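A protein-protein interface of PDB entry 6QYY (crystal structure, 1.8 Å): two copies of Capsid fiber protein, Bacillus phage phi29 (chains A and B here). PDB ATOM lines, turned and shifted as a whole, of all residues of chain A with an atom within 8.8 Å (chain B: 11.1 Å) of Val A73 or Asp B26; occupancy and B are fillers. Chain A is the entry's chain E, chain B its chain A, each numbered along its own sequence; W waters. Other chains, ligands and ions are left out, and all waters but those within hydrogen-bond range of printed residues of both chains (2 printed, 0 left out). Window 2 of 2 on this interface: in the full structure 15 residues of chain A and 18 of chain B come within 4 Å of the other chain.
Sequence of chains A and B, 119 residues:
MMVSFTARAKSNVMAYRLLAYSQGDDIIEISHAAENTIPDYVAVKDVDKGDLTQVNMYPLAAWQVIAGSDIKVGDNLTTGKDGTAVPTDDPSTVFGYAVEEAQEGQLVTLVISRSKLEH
The side-chain amide nitrogen (NE2) of Gln B23 is in hydrogen-bond range of the backbone carbonyl oxygen (O) of Val A73 (3.5 Å).
N of Val A99 is in hydrogen-bond range of O of Thr A109 (3.0 Å). The backbone carbonyl oxygen (O) of Ile B28 sits at hydrogen-bond distance from the backbone NH (N) of Arg B8 (3.0 Å). The backbone carbonyl oxygen (O) of Ala A98 lies within hydrogen-bond range of the backbone NH (N) of Gly A74, at 2.8 Å.
Asp B26 touches Val A73 (O to CG2, 3.8 Å). Val A73 touches Ile B27 (CG1 to C, 3.8 Å). CG1 of Val A73 touches CG1 of Ile B28, 3.6 Å away. CA of Gly A74 touches NE2 of Gln B23 (3.3 Å). OH of Tyr A97 touches CD2 of Tyr B21 (3.5 Å). Val A99 touches Phe B5. Ile B28 touches Val A99 (CG1 to CA, 3.6 Å).
Lys A72 touches none of the printed residues of chain B. Of the printed residues of chain B, Val A73 touches Gln B23 (3.5 Å), Asp B26 (3.8 Å), Ile B27 (3.8 Å) and Ile B28 (3.6 Å). Gly A74 touches just one residue of chain B: Gln B23 (3.3 Å). No residue of chain B comes within 4 Å of Asp A75. Of the printed residues of chain B, Tyr A97 touches Tyr B21. No residue of chain B comes within 4 Å of Glu A101. Thr A109 touches none of the printed residues of chain B. Printed residues of chain A within 4 Å of Phe B5: Val A99. Printed residues of chain A within 4 Å of Tyr B21: Tyr A97 (3.5 Å). Of the printed residues of chain A, Gln B23 touches Val A73 and Gly A74. Of the printed residues of chain A, Asp B26 touches Val A73. Printed residues of chain A within 4 Å of Ile B28: Val A73 and Val A99. The nearest residue of chain B that does not touch Val A73 is Gly B24 (5.9 Å). The nearest printed residue of chain A that does not touch Phe B5 is Glu A100 (4.03 Å).
Of the 15 printed residues of chain B, 6 touch a printed residue of chain A. Printed residues of chain B that touch a printed residue of chain A: Phe B5, Tyr B21, Gln B23, Asp B26, Ile B27 and Ile B28. Hydrophobic or aromatic side chains of chain B within 4 Å of the printed part of chain A: Phe B5, Tyr B21 and Ile B28. Printed residues of chain A that touch a printed residue of chain B: Val A73, Gly A74, Tyr A97 and Val A99. Hydrophobic or aromatic side chains of chain A that line the printed part of chain B: Val A73, Tyr A97 and Val A99. Among the printed residues, 8 pairs touch across the chains. Among the printed residues, no Asp or Glu carboxylate lies within 4 Å of a Lys or Arg side-chain nitrogen of the other chain.
No position is printed for both chains. Of the 8 pairs that touch across the chains among the printed residues, none has its exchanged pair printed and touching as well.
Water W2 lies within hydrogen-bond range of the backbone carbonyl oxygen of Val A73 and the side-chain amide oxygen of Gln B23. Water W1 lies within hydrogen-bond range of the backbone NH of Thr B6 (2.8 Å) and the side-chain carboxylate of Glu A100 (2.9 Å).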
ATOM      1  N   ASP A  70      17.422  -0.240 -20.084  1.00  0.00           N
ATOM      2  CA  ASP A  70      18.642  -1.024 -20.041  1.00  0.00           C
ATOM      3  C   ASP A  70      18.439  -2.359 -20.757  1.00  0.00           C
ATOM      4  O   ASP A  70      17.385  -2.987 -20.668  1.00  0.00           O
ATOM      5  CB  ASP A  70      19.120  -1.215 -18.592  1.00  0.00           C
ATOM      6  CG  ASP A  70      19.420   0.116 -17.884  1.00  0.00           C
ATOM      7  OD1 ASP A  70      19.429   1.182 -18.546  1.00  0.00           O
ATOM      8  OD2 ASP A  70      19.680   0.105 -16.667  1.00  0.00           O
ATOM      9  N   ILE A  71      19.448  -2.758 -21.510  1.00  0.00           N
ATOM     10  CA  ILE A  71      19.387  -3.906 -22.403  1.00  0.00           C
ATOM     11  C   ILE A  71      20.595  -4.784 -22.110  1.00  0.00           C
ATOM     12  O   ILE A  71      21.719  -4.276 -21.992  1.00  0.00           O
ATOM     13  CB  ILE A  71      19.394  -3.468 -23.881  1.00  0.00           C
ATOM     14  CG1 ILE A  71      18.077  -2.791 -24.246  1.00  0.00           C
ATOM     15  CG2 ILE A  71      19.650  -4.650 -24.807  1.00  0.00           C
ATOM     16  CD1 ILE A  71      18.075  -2.249 -25.652  1.00  0.00           C
ATOM     17  N   LYS A  72      20.363  -6.090 -21.980  1.00  0.00           N
ATOM     18  CA  LYS A  72      21.427  -7.069 -21.801  1.00  0.00           C
ATOM     19  C   LYS A  72      21.645  -7.844 -23.093  1.00  0.00           C
ATOM     20  O   LYS A  72      20.744  -7.960 -23.929  1.00  0.00           O
ATOM     21  CB  LYS A  72      21.093  -8.042 -20.665  1.00  0.00           C
ATOM     22  CG  LYS A  72      21.137  -7.426 -19.280  1.00  0.00           C
ATOM     23  CD  LYS A  72      20.890  -8.480 -18.211  1.00  0.00           C
ATOM     24  CE  LYS A  72      21.246  -7.963 -16.823  1.00  0.00           C
ATOM     25  NZ  LYS A  72      21.322  -9.052 -15.809  1.00  0.00           N
ATOM     26  N   VAL A  73      22.864  -8.369 -23.253  1.00  0.00           N
ATOM     27  CA  VAL A  73      23.183  -9.150 -24.442  1.00  0.00           C
ATOM     28  C   VAL A  73      22.197 -10.304 -24.576  1.00  0.00           C
ATOM     29  O   VAL A  73      21.907 -11.014 -23.604  1.00  0.00           O
ATOM     30  CB  VAL A  73      24.622  -9.684 -24.366  1.00  0.00           C
ATOM     31  CG1 VAL A  73      24.901 -10.588 -25.550  1.00  0.00           C
ATOM     32  CG2 VAL A  73      25.615  -8.551 -24.285  1.00  0.00           C
ATOM     33  N   GLY A  74      21.671 -10.491 -25.781  1.00  0.00           N
ATOM     34  CA  GLY A  74      20.723 -11.554 -26.041  1.00  0.00           C
ATOM     35  C   GLY A  74      19.262 -11.213 -25.796  1.00  0.00           C
ATOM     36  O   GLY A  74      18.394 -12.032 -26.132  1.00  0.00           O
ATOM     37  N   ASP A  75      18.963 -10.049 -25.212  1.00  0.00           N
ATOM     38  CA  ASP A  75      17.580  -9.657 -24.986  1.00  0.00           C
ATOM     39  C   ASP A  75      16.852  -9.579 -26.314  1.00  0.00           C
ATOM     40  O   ASP A  75      17.362  -9.005 -27.276  1.00  0.00           O
ATOM     41  CB  ASP A  75      17.494  -8.282 -24.313  1.00  0.00           C
ATOM     42  CG  ASP A  75      17.660  -8.326 -22.801  1.00  0.00           C
ATOM     43  OD1 ASP A  75      17.698  -9.419 -22.204  1.00  0.00           O
ATOM     44  OD2 ASP A  75      17.762  -7.226 -22.212  1.00  0.00           O
ATOM     45  N   ASN A  76      15.622 -10.092 -26.351  1.00  0.00           N
ATOM     46  CA  ASN A  76      14.789  -9.865 -27.522  1.00  0.00           C
ATOM     47  C   ASN A  76      14.175  -8.480 -27.448  1.00  0.00           C
ATOM     48  O   ASN A  76      13.709  -8.052 -26.390  1.00  0.00           O
ATOM     49  CB  ASN A  76      13.700 -10.934 -27.639  1.00  0.00           C
ATOM     50  CG  ASN A  76      14.273 -12.327 -27.702  1.00  0.00           C
ATOM     51  OD1 ASN A  76      14.955 -12.679 -28.671  1.00  0.00           O
ATOM     52  ND2 ASN A  76      13.966 -13.141 -26.700  1.00  0.00           N
ATOM     53  N   LEU A  77      14.174  -7.779 -28.582  1.00  0.00           N
ATOM     54  CA  LEU A  77      13.863  -6.361 -28.606  1.00  0.00           C
ATOM     55  C   LEU A  77      12.634  -6.073 -29.450  1.00  0.00           C
ATOM     56  O   LEU A  77      12.410  -6.709 -30.487  1.00  0.00           O
ATOM     57  CB  LEU A  77      15.039  -5.552 -29.171  1.00  0.00           C
ATOM     58  CG  LEU A  77      16.366  -5.737 -28.425  1.00  0.00           C
ATOM     59  CD1 LEU A  77      17.414  -4.878 -29.137  1.00  0.00           C
ATOM     60  CD2 LEU A  77      16.247  -5.344 -26.971  1.00  0.00           C
ATOM     61  N   PRO A  87      13.705  -4.270 -24.377  1.00  0.00           N
ATOM     62  CA  PRO A  87      13.418  -5.702 -24.257  1.00  0.00           C
ATOM     63  C   PRO A  87      11.920  -5.965 -24.170  1.00  0.00           C
ATOM     64  O   PRO A  87      11.151  -5.140 -23.673  1.00  0.00           O
ATOM     65  CB  PRO A  87      14.108  -6.101 -22.943  1.00  0.00           C
ATOM     66  CG  PRO A  87      15.086  -4.999 -22.662  1.00  0.00           C
ATOM     67  CD  PRO A  87      14.452  -3.764 -23.212  1.00  0.00           C
ATOM     68  N   TYR A  97      17.460  -9.208 -31.692  1.00  0.00           N
ATOM     69  CA  TYR A  97      18.034  -9.426 -30.366  1.00  0.00           C
ATOM     70  C   TYR A  97      19.324  -8.634 -30.213  1.00  0.00           C
ATOM     71  O   TYR A  97      20.065  -8.439 -31.173  1.00  0.00           O
ATOM     72  CB  TYR A  97      18.304 -10.913 -30.059  1.00  0.00           C
ATOM     73  CG  TYR A  97      19.211 -11.608 -31.042  1.00  0.00           C
ATOM     74  CD1 TYR A  97      20.600 -11.652 -30.842  1.00  0.00           C
ATOM     75  CD2 TYR A  97      18.688 -12.229 -32.175  1.00  0.00           C
ATOM     76  CE1 TYR A  97      21.440 -12.302 -31.765  1.00  0.00           C
ATOM     77  CE2 TYR A  97      19.517 -12.872 -33.100  1.00  0.00           C
ATOM     78  CZ  TYR A  97      20.886 -12.908 -32.882  1.00  0.00           C
ATOM     79  OH  TYR A  97      21.694 -13.546 -33.787  1.00  0.00           O
ATOM     80  N   ALA A  98      19.568  -8.163 -28.991  1.00  0.00           N
ATOM     81  CA  ALA A  98      20.742  -7.347 -28.721  1.00  0.00           C
ATOM     82  C   ALA A  98      22.004  -8.193 -28.777  1.00  0.00           C
ATOM     83  O   ALA A  98      22.032  -9.311 -28.260  1.00  0.00           O
ATOM     84  CB  ALA A  98      20.626  -6.701 -27.346  1.00  0.00           C
ATOM     85  N   VAL A  99      23.054  -7.661 -29.412  1.00  0.00           N
ATOM     86  CA  VAL A  99      24.350  -8.329 -29.397  1.00  0.00           C
ATOM     87  C   VAL A  99      25.353  -7.590 -28.533  1.00  0.00           C
ATOM     88  O   VAL A  99      26.545  -7.917 -28.550  1.00  0.00           O
ATOM     89  CB  VAL A  99      24.908  -8.561 -30.809  1.00  0.00           C
ATOM     90  CG1 VAL A  99      24.032  -9.583 -31.534  1.00  0.00           C
ATOM     91  CG2 VAL A  99      25.073  -7.234 -31.575  1.00  0.00           C
ATOM     92  N   GLU A 100      24.894  -6.617 -27.752  1.00  0.00           N
ATOM     93  CA  GLU A 100      25.737  -5.996 -26.744  1.00  0.00           C
ATOM     94  C   GLU A 100      24.844  -5.378 -25.681  1.00  0.00           C
ATOM     95  O   GLU A 100      23.646  -5.180 -25.889  1.00  0.00           O
ATOM     96  CB  GLU A 100      26.664  -4.943 -27.353  1.00  0.00           C
ATOM     97  CG  GLU A 100      25.924  -3.754 -27.855  1.00  0.00           C
ATOM     98  CD  GLU A 100      26.747  -2.926 -28.820  1.00  0.00           C
ATOM     99  OE1 GLU A 100      26.192  -1.916 -29.300  1.00  0.00           O
ATOM    100  OE2 GLU A 100      27.929  -3.273 -29.087  1.00  0.00           O
ATOM    101  N   GLU A 101      25.446  -5.092 -24.534  1.00  0.00           N
ATOM    102  CA  GLU A 101      24.751  -4.398 -23.462  1.00  0.00           C
ATOM    103  C   GLU A 101      24.577  -2.919 -23.807  1.00  0.00           C
ATOM    104  O   GLU A 101      25.413  -2.316 -24.484  1.00  0.00           O
ATOM    105  CB  GLU A 101      25.545  -4.537 -22.168  1.00  0.00           C
ATOM    106  CG  GLU A 101      24.764  -4.331 -20.906  1.00  0.00           C
ATOM    107  CD  GLU A 101      25.585  -4.691 -19.688  1.00  0.00           C
ATOM    108  OE1 GLU A 101      25.862  -5.897 -19.493  1.00  0.00           O
ATOM    109  OE2 GLU A 101      25.969  -3.765 -18.942  1.00  0.00           O
ATOM    110  N   ALA A 102      23.496  -2.324 -23.305  1.00  0.00           N
ATOM    111  CA  ALA A 102      23.285  -0.893 -23.458  1.00  0.00           C
ATOM    112  C   ALA A 102      22.442  -0.375 -22.305  1.00  0.00           C
ATOM    113  O   ALA A 102      21.500  -1.040 -21.862  1.00  0.00           O
ATOM    114  CB  ALA A 102      22.610  -0.566 -24.794  1.00  0.00           C
ATOM    115  N   VAL A 108      22.547   0.810 -29.139  1.00  0.00           N
ATOM    116  CA  VAL A 108      22.677  -0.632 -28.998  1.00  0.00           C
ATOM    117  C   VAL A 108      22.695  -1.264 -30.380  1.00  0.00           C
ATOM    118  O   VAL A 108      21.985  -0.833 -31.296  1.00  0.00           O
ATOM    119  CB  VAL A 108      21.561  -1.247 -28.121  1.00  0.00           C
ATOM    120  CG1 VAL A 108      20.219  -1.180 -28.805  1.00  0.00           C
ATOM    121  CG2 VAL A 108      21.902  -2.691 -27.755  1.00  0.00           C
ATOM    122  N   THR A 109      23.532  -2.274 -30.536  1.00  0.00           N
ATOM    123  CA  THR A 109      23.612  -3.020 -31.770  1.00  0.00           C
ATOM    124  C   THR A 109      22.757  -4.266 -31.626  1.00  0.00           C
ATOM    125  O   THR A 109      22.741  -4.905 -30.569  1.00  0.00           O
ATOM    126  CB  THR A 109      25.060  -3.379 -32.086  1.00  0.00           C
ATOM    127  OG1 THR A 109      25.827  -2.168 -32.109  1.00  0.00           O
ATOM    128  CG2 THR A 109      25.167  -4.083 -33.402  1.00  0.00           C
ATOM    129  N   PHE B   5      30.393  -5.107 -33.532  1.00  0.00           N
ATOM    130  CA  PHE B   5      30.205  -5.486 -32.140  1.00  0.00           C
ATOM    131  C   PHE B   5      31.284  -6.488 -31.749  1.00  0.00           C
ATOM    132  O   PHE B   5      31.924  -7.117 -32.598  1.00  0.00           O
ATOM    133  CB  PHE B   5      28.795  -6.048 -31.883  1.00  0.00           C
ATOM    134  CG  PHE B   5      28.522  -7.413 -32.499  1.00  0.00           C
ATOM    135  CD1 PHE B   5      28.683  -8.574 -31.747  1.00  0.00           C
ATOM    136  CD2 PHE B   5      28.038  -7.526 -33.798  1.00  0.00           C
ATOM    137  CE1 PHE B   5      28.407  -9.823 -32.293  1.00  0.00           C
ATOM    138  CE2 PHE B   5      27.764  -8.771 -34.357  1.00  0.00           C
ATOM    139  CZ  PHE B   5      27.953  -9.925 -33.606  1.00  0.00           C
ATOM    140  N   THR B   6      31.499  -6.618 -30.447  1.00  0.00           N
ATOM    141  CA  THR B   6      32.519  -7.528 -29.951  1.00  0.00           C
ATOM    142  C   THR B   6      31.879  -8.859 -29.585  1.00  0.00           C
ATOM    143  O   THR B   6      30.773  -8.904 -29.035  1.00  0.00           O
ATOM    144  CB  THR B   6      33.250  -6.907 -28.758  1.00  0.00           C
ATOM    145  OG1 THR B   6      34.001  -5.783 -29.237  1.00  0.00           O
ATOM    146  CG2 THR B   6      34.224  -7.913 -28.109  1.00  0.00           C
ATOM    147  N   ALA B   7      32.563  -9.939 -29.940  1.00  0.00           N
ATOM    148  CA  ALA B   7      32.102 -11.283 -29.657  1.00  0.00           C
ATOM    149  C   ALA B   7      33.281 -12.084 -29.134  1.00  0.00           C
ATOM    150  O   ALA B   7      34.437 -11.678 -29.261  1.00  0.00           O
ATOM    151  CB  ALA B   7      31.511 -11.937 -30.911  1.00  0.00           C
ATOM    152  N   ARG B   8      32.981 -13.229 -28.544  1.00  0.00           N
ATOM    153  CA  ARG B   8      34.002 -14.175 -28.119  1.00  0.00           C
ATOM    154  C   ARG B   8      33.811 -15.451 -28.922  1.00  0.00           C
ATOM    155  O   ARG B   8      32.685 -15.914 -29.096  1.00  0.00           O
ATOM    156  CB  ARG B   8      33.913 -14.461 -26.609  1.00  0.00           C
ATOM    157  CG  ARG B   8      35.029 -15.348 -26.093  1.00  0.00           C
ATOM    158  CD  ARG B   8      35.014 -15.479 -24.568  1.00  0.00           C
ATOM    159  NE  ARG B   8      34.956 -14.197 -23.856  1.00  0.00           N
ATOM    160  CZ  ARG B   8      36.015 -13.464 -23.517  1.00  0.00           C
ATOM    161  NH1 ARG B   8      37.239 -13.859 -23.840  1.00  0.00           N
ATOM    162  NH2 ARG B   8      35.851 -12.325 -22.858  1.00  0.00           N
ATOM    163  N   TYR B  21      25.539 -17.090 -34.203  1.00  0.00           N
ATOM    164  CA  TYR B  21      25.645 -16.305 -32.986  1.00  0.00           C
ATOM    165  C   TYR B  21      24.948 -17.048 -31.855  1.00  0.00           C
ATOM    166  O   TYR B  21      23.880 -17.633 -32.052  1.00  0.00           O
ATOM    167  CB  TYR B  21      25.014 -14.932 -33.173  1.00  0.00           C
ATOM    168  CG  TYR B  21      25.677 -14.072 -34.207  1.00  0.00           C
ATOM    169  CD1 TYR B  21      26.976 -14.331 -34.634  1.00  0.00           C
ATOM    170  CD2 TYR B  21      24.996 -12.996 -34.772  1.00  0.00           C
ATOM    171  CE1 TYR B  21      27.595 -13.502 -35.589  1.00  0.00           C
ATOM    172  CE2 TYR B  21      25.606 -12.175 -35.705  1.00  0.00           C
ATOM    173  CZ  TYR B  21      26.890 -12.430 -36.116  1.00  0.00           C
ATOM    174  OH  TYR B  21      27.471 -11.598 -37.045  1.00  0.00           O
ATOM    175  N   SER B  22      25.545 -17.013 -30.667  1.00  0.00           N
ATOM    176  CA  SER B  22      24.935 -17.714 -29.547  1.00  0.00           C
ATOM    177  C   SER B  22      25.152 -16.918 -28.273  1.00  0.00           C
ATOM    178  O   SER B  22      26.035 -16.058 -28.185  1.00  0.00           O
ATOM    179  CB  SER B  22      25.478 -19.142 -29.403  1.00  0.00           C
ATOM    180  OG  SER B  22      26.795 -19.126 -28.894  1.00  0.00           O
ATOM    181  N   GLN B  23      24.317 -17.223 -27.287  1.00  0.00           N
ATOM    182  CA  GLN B  23      24.345 -16.564 -25.991  1.00  0.00           C
ATOM    183  C   GLN B  23      25.515 -17.099 -25.173  1.00  0.00           C
ATOM    184  O   GLN B  23      25.558 -18.290 -24.856  1.00  0.00           O
ATOM    185  CB  GLN B  23      23.018 -16.814 -25.269  1.00  0.00           C
ATOM    186  CG  GLN B  23      22.872 -16.153 -23.915  1.00  0.00           C
ATOM    187  CD  GLN B  23      23.056 -14.652 -23.969  1.00  0.00           C
ATOM    188  OE1 GLN B  23      23.535 -14.045 -23.017  1.00  0.00           O
ATOM    189  NE2 GLN B  23      22.662 -14.041 -25.083  1.00  0.00           N
ATOM    190  N   GLY B  24      26.466 -16.229 -24.849  1.00  0.00           N
ATOM    191  CA  GLY B  24      27.509 -16.536 -23.896  1.00  0.00           C
ATOM    192  C   GLY B  24      27.276 -15.846 -22.568  1.00  0.00           C
ATOM    193  O   GLY B  24      26.161 -15.423 -22.242  1.00  0.00           O
ATOM    194  N   ASP B  25      28.348 -15.710 -21.795  1.00  0.00           N
ATOM    195  CA  ASP B  25      28.274 -15.046 -20.493  1.00  0.00           C
ATOM    196  C   ASP B  25      28.539 -13.555 -20.686  1.00  0.00           C
ATOM    197  O   ASP B  25      29.683 -13.138 -20.880  1.00  0.00           O
ATOM    198  CB  ASP B  25      29.266 -15.668 -19.517  1.00  0.00           C
ATOM    199  CG  ASP B  25      28.696 -15.808 -18.120  1.00  0.00           C
ATOM    200  OD1 ASP B  25      28.830 -16.897 -17.522  1.00  0.00           O
ATOM    201  OD2 ASP B  25      28.101 -14.826 -17.623  1.00  0.00           O
ATOM    202  N   ASP B  26      27.475 -12.747 -20.630  1.00  0.00           N
ATOM    203  CA  ASP B  26      27.552 -11.297 -20.824  1.00  0.00           C
ATOM    204  C   ASP B  26      28.139 -10.920 -22.183  1.00  0.00           C
ATOM    205  O   ASP B  26      28.612  -9.795 -22.368  1.00  0.00           O
ATOM    206  CB  ASP B  26      28.361 -10.621 -19.710  1.00  0.00           C
ATOM    207  CG  ASP B  26      27.520 -10.266 -18.513  1.00  0.00           C
ATOM    208  OD1 ASP B  26      26.508 -10.954 -18.274  1.00  0.00           O
ATOM    209  OD2 ASP B  26      27.875  -9.297 -17.806  1.00  0.00           O
ATOM    210  N   ILE B  27      28.117 -11.833 -23.152  1.00  0.00           N
ATOM    211  CA  ILE B  27      28.723 -11.574 -24.452  1.00  0.00           C
ATOM    212  C   ILE B  27      28.126 -12.544 -25.457  1.00  0.00           C
ATOM    213  O   ILE B  27      27.700 -13.649 -25.099  1.00  0.00           O
ATOM    214  CB  ILE B  27      30.266 -11.697 -24.382  1.00  0.00           C
ATOM    215  CG1 ILE B  27      30.910 -10.987 -25.568  1.00  0.00           C
ATOM    216  CG2 ILE B  27      30.710 -13.178 -24.279  1.00  0.00           C
ATOM    217  CD1 ILE B  27      32.380 -10.737 -25.378  1.00  0.00           C
ATOM    218  N   ILE B  28      28.063 -12.110 -26.719  1.00  0.00           N
ATOM    219  CA  ILE B  28      27.687 -12.988 -27.818  1.00  0.00           C
ATOM    220  C   ILE B  28      28.875 -13.862 -28.143  1.00  0.00           C
ATOM    221  O   ILE B  28      30.012 -13.385 -28.201  1.00  0.00           O
ATOM    222  CB  ILE B  28      27.252 -12.188 -29.061  1.00  0.00           C
ATOM    223  CG1 ILE B  28      25.885 -11.566 -28.855  1.00  0.00           C
ATOM    224  CG2 ILE B  28      27.169 -13.095 -30.288  1.00  0.00           C
ATOM    225  CD1 ILE B  28      24.748 -12.585 -28.647  1.00  0.00           C
ATOM    226  N   GLU B  29      28.628 -15.149 -28.335  1.00  0.00           N
ATOM    227  CA  GLU B  29      29.671 -16.048 -28.789  1.00  0.00           C
ATOM    228  C   GLU B  29      29.439 -16.395 -30.254  1.00  0.00           C
ATOM    229  O   GLU B  29      28.300 -16.430 -30.725  1.00  0.00           O
ATOM    230  CB  GLU B  29      29.739 -17.299 -27.901  1.00  0.00           C
ATOM    231  CG  GLU B  29      30.103 -16.937 -26.463  1.00  0.00           C
ATOM    232  CD  GLU B  29      30.425 -18.136 -25.584  1.00  0.00           C
ATOM    233  OE1 GLU B  29      31.239 -17.988 -24.641  1.00  0.00           O
ATOM    234  OE2 GLU B  29      29.852 -19.221 -25.823  1.00  0.00           O
ATOM    235  N   ILE B  30      30.528 -16.573 -30.990  1.00  0.00           N
ATOM    236  CA  ILE B  30      30.451 -17.013 -32.374  1.00  0.00           C
ATOM    237  C   ILE B  30      31.097 -18.386 -32.488  1.00  0.00           C
ATOM    238  O   ILE B  30      31.980 -18.763 -31.705  1.00  0.00           O
ATOM    239  CB  ILE B  30      31.125 -16.019 -33.345  1.00  0.00           C
ATOM    240  CG1 ILE B  30      32.591 -15.830 -32.979  1.00  0.00           C
ATOM    241  CG2 ILE B  30      30.379 -14.670 -33.382  1.00  0.00           C
ATOM    242  CD1 ILE B  30      33.388 -15.070 -34.057  1.00  0.00           C
ATOM    243  N   LEU B  52      38.561 -12.765 -27.904  1.00  0.00           N
ATOM    244  CA  LEU B  52      37.664 -11.723 -28.367  1.00  0.00           C
ATOM    245  C   LEU B  52      37.940 -11.407 -29.827  1.00  0.00           C
ATOM    246  O   LEU B  52      39.028 -11.659 -30.352  1.00  0.00           O
ATOM    247  CB  LEU B  52      37.815 -10.457 -27.535  1.00  0.00           C
ATOM    248  CG  LEU B  52      37.404 -10.622 -26.087  1.00  0.00           C
ATOM    249  CD1 LEU B  52      37.870  -9.436 -25.282  1.00  0.00           C
ATOM    250  CD2 LEU B  52      35.901 -10.776 -26.021  1.00  0.00           C
HETATM  251  O   HOH W   1      30.237  -4.903 -28.565  1.00  0.00           O
HETATM  252  O   HOH W   2      23.128 -11.282 -21.140  1.00  0.00           O
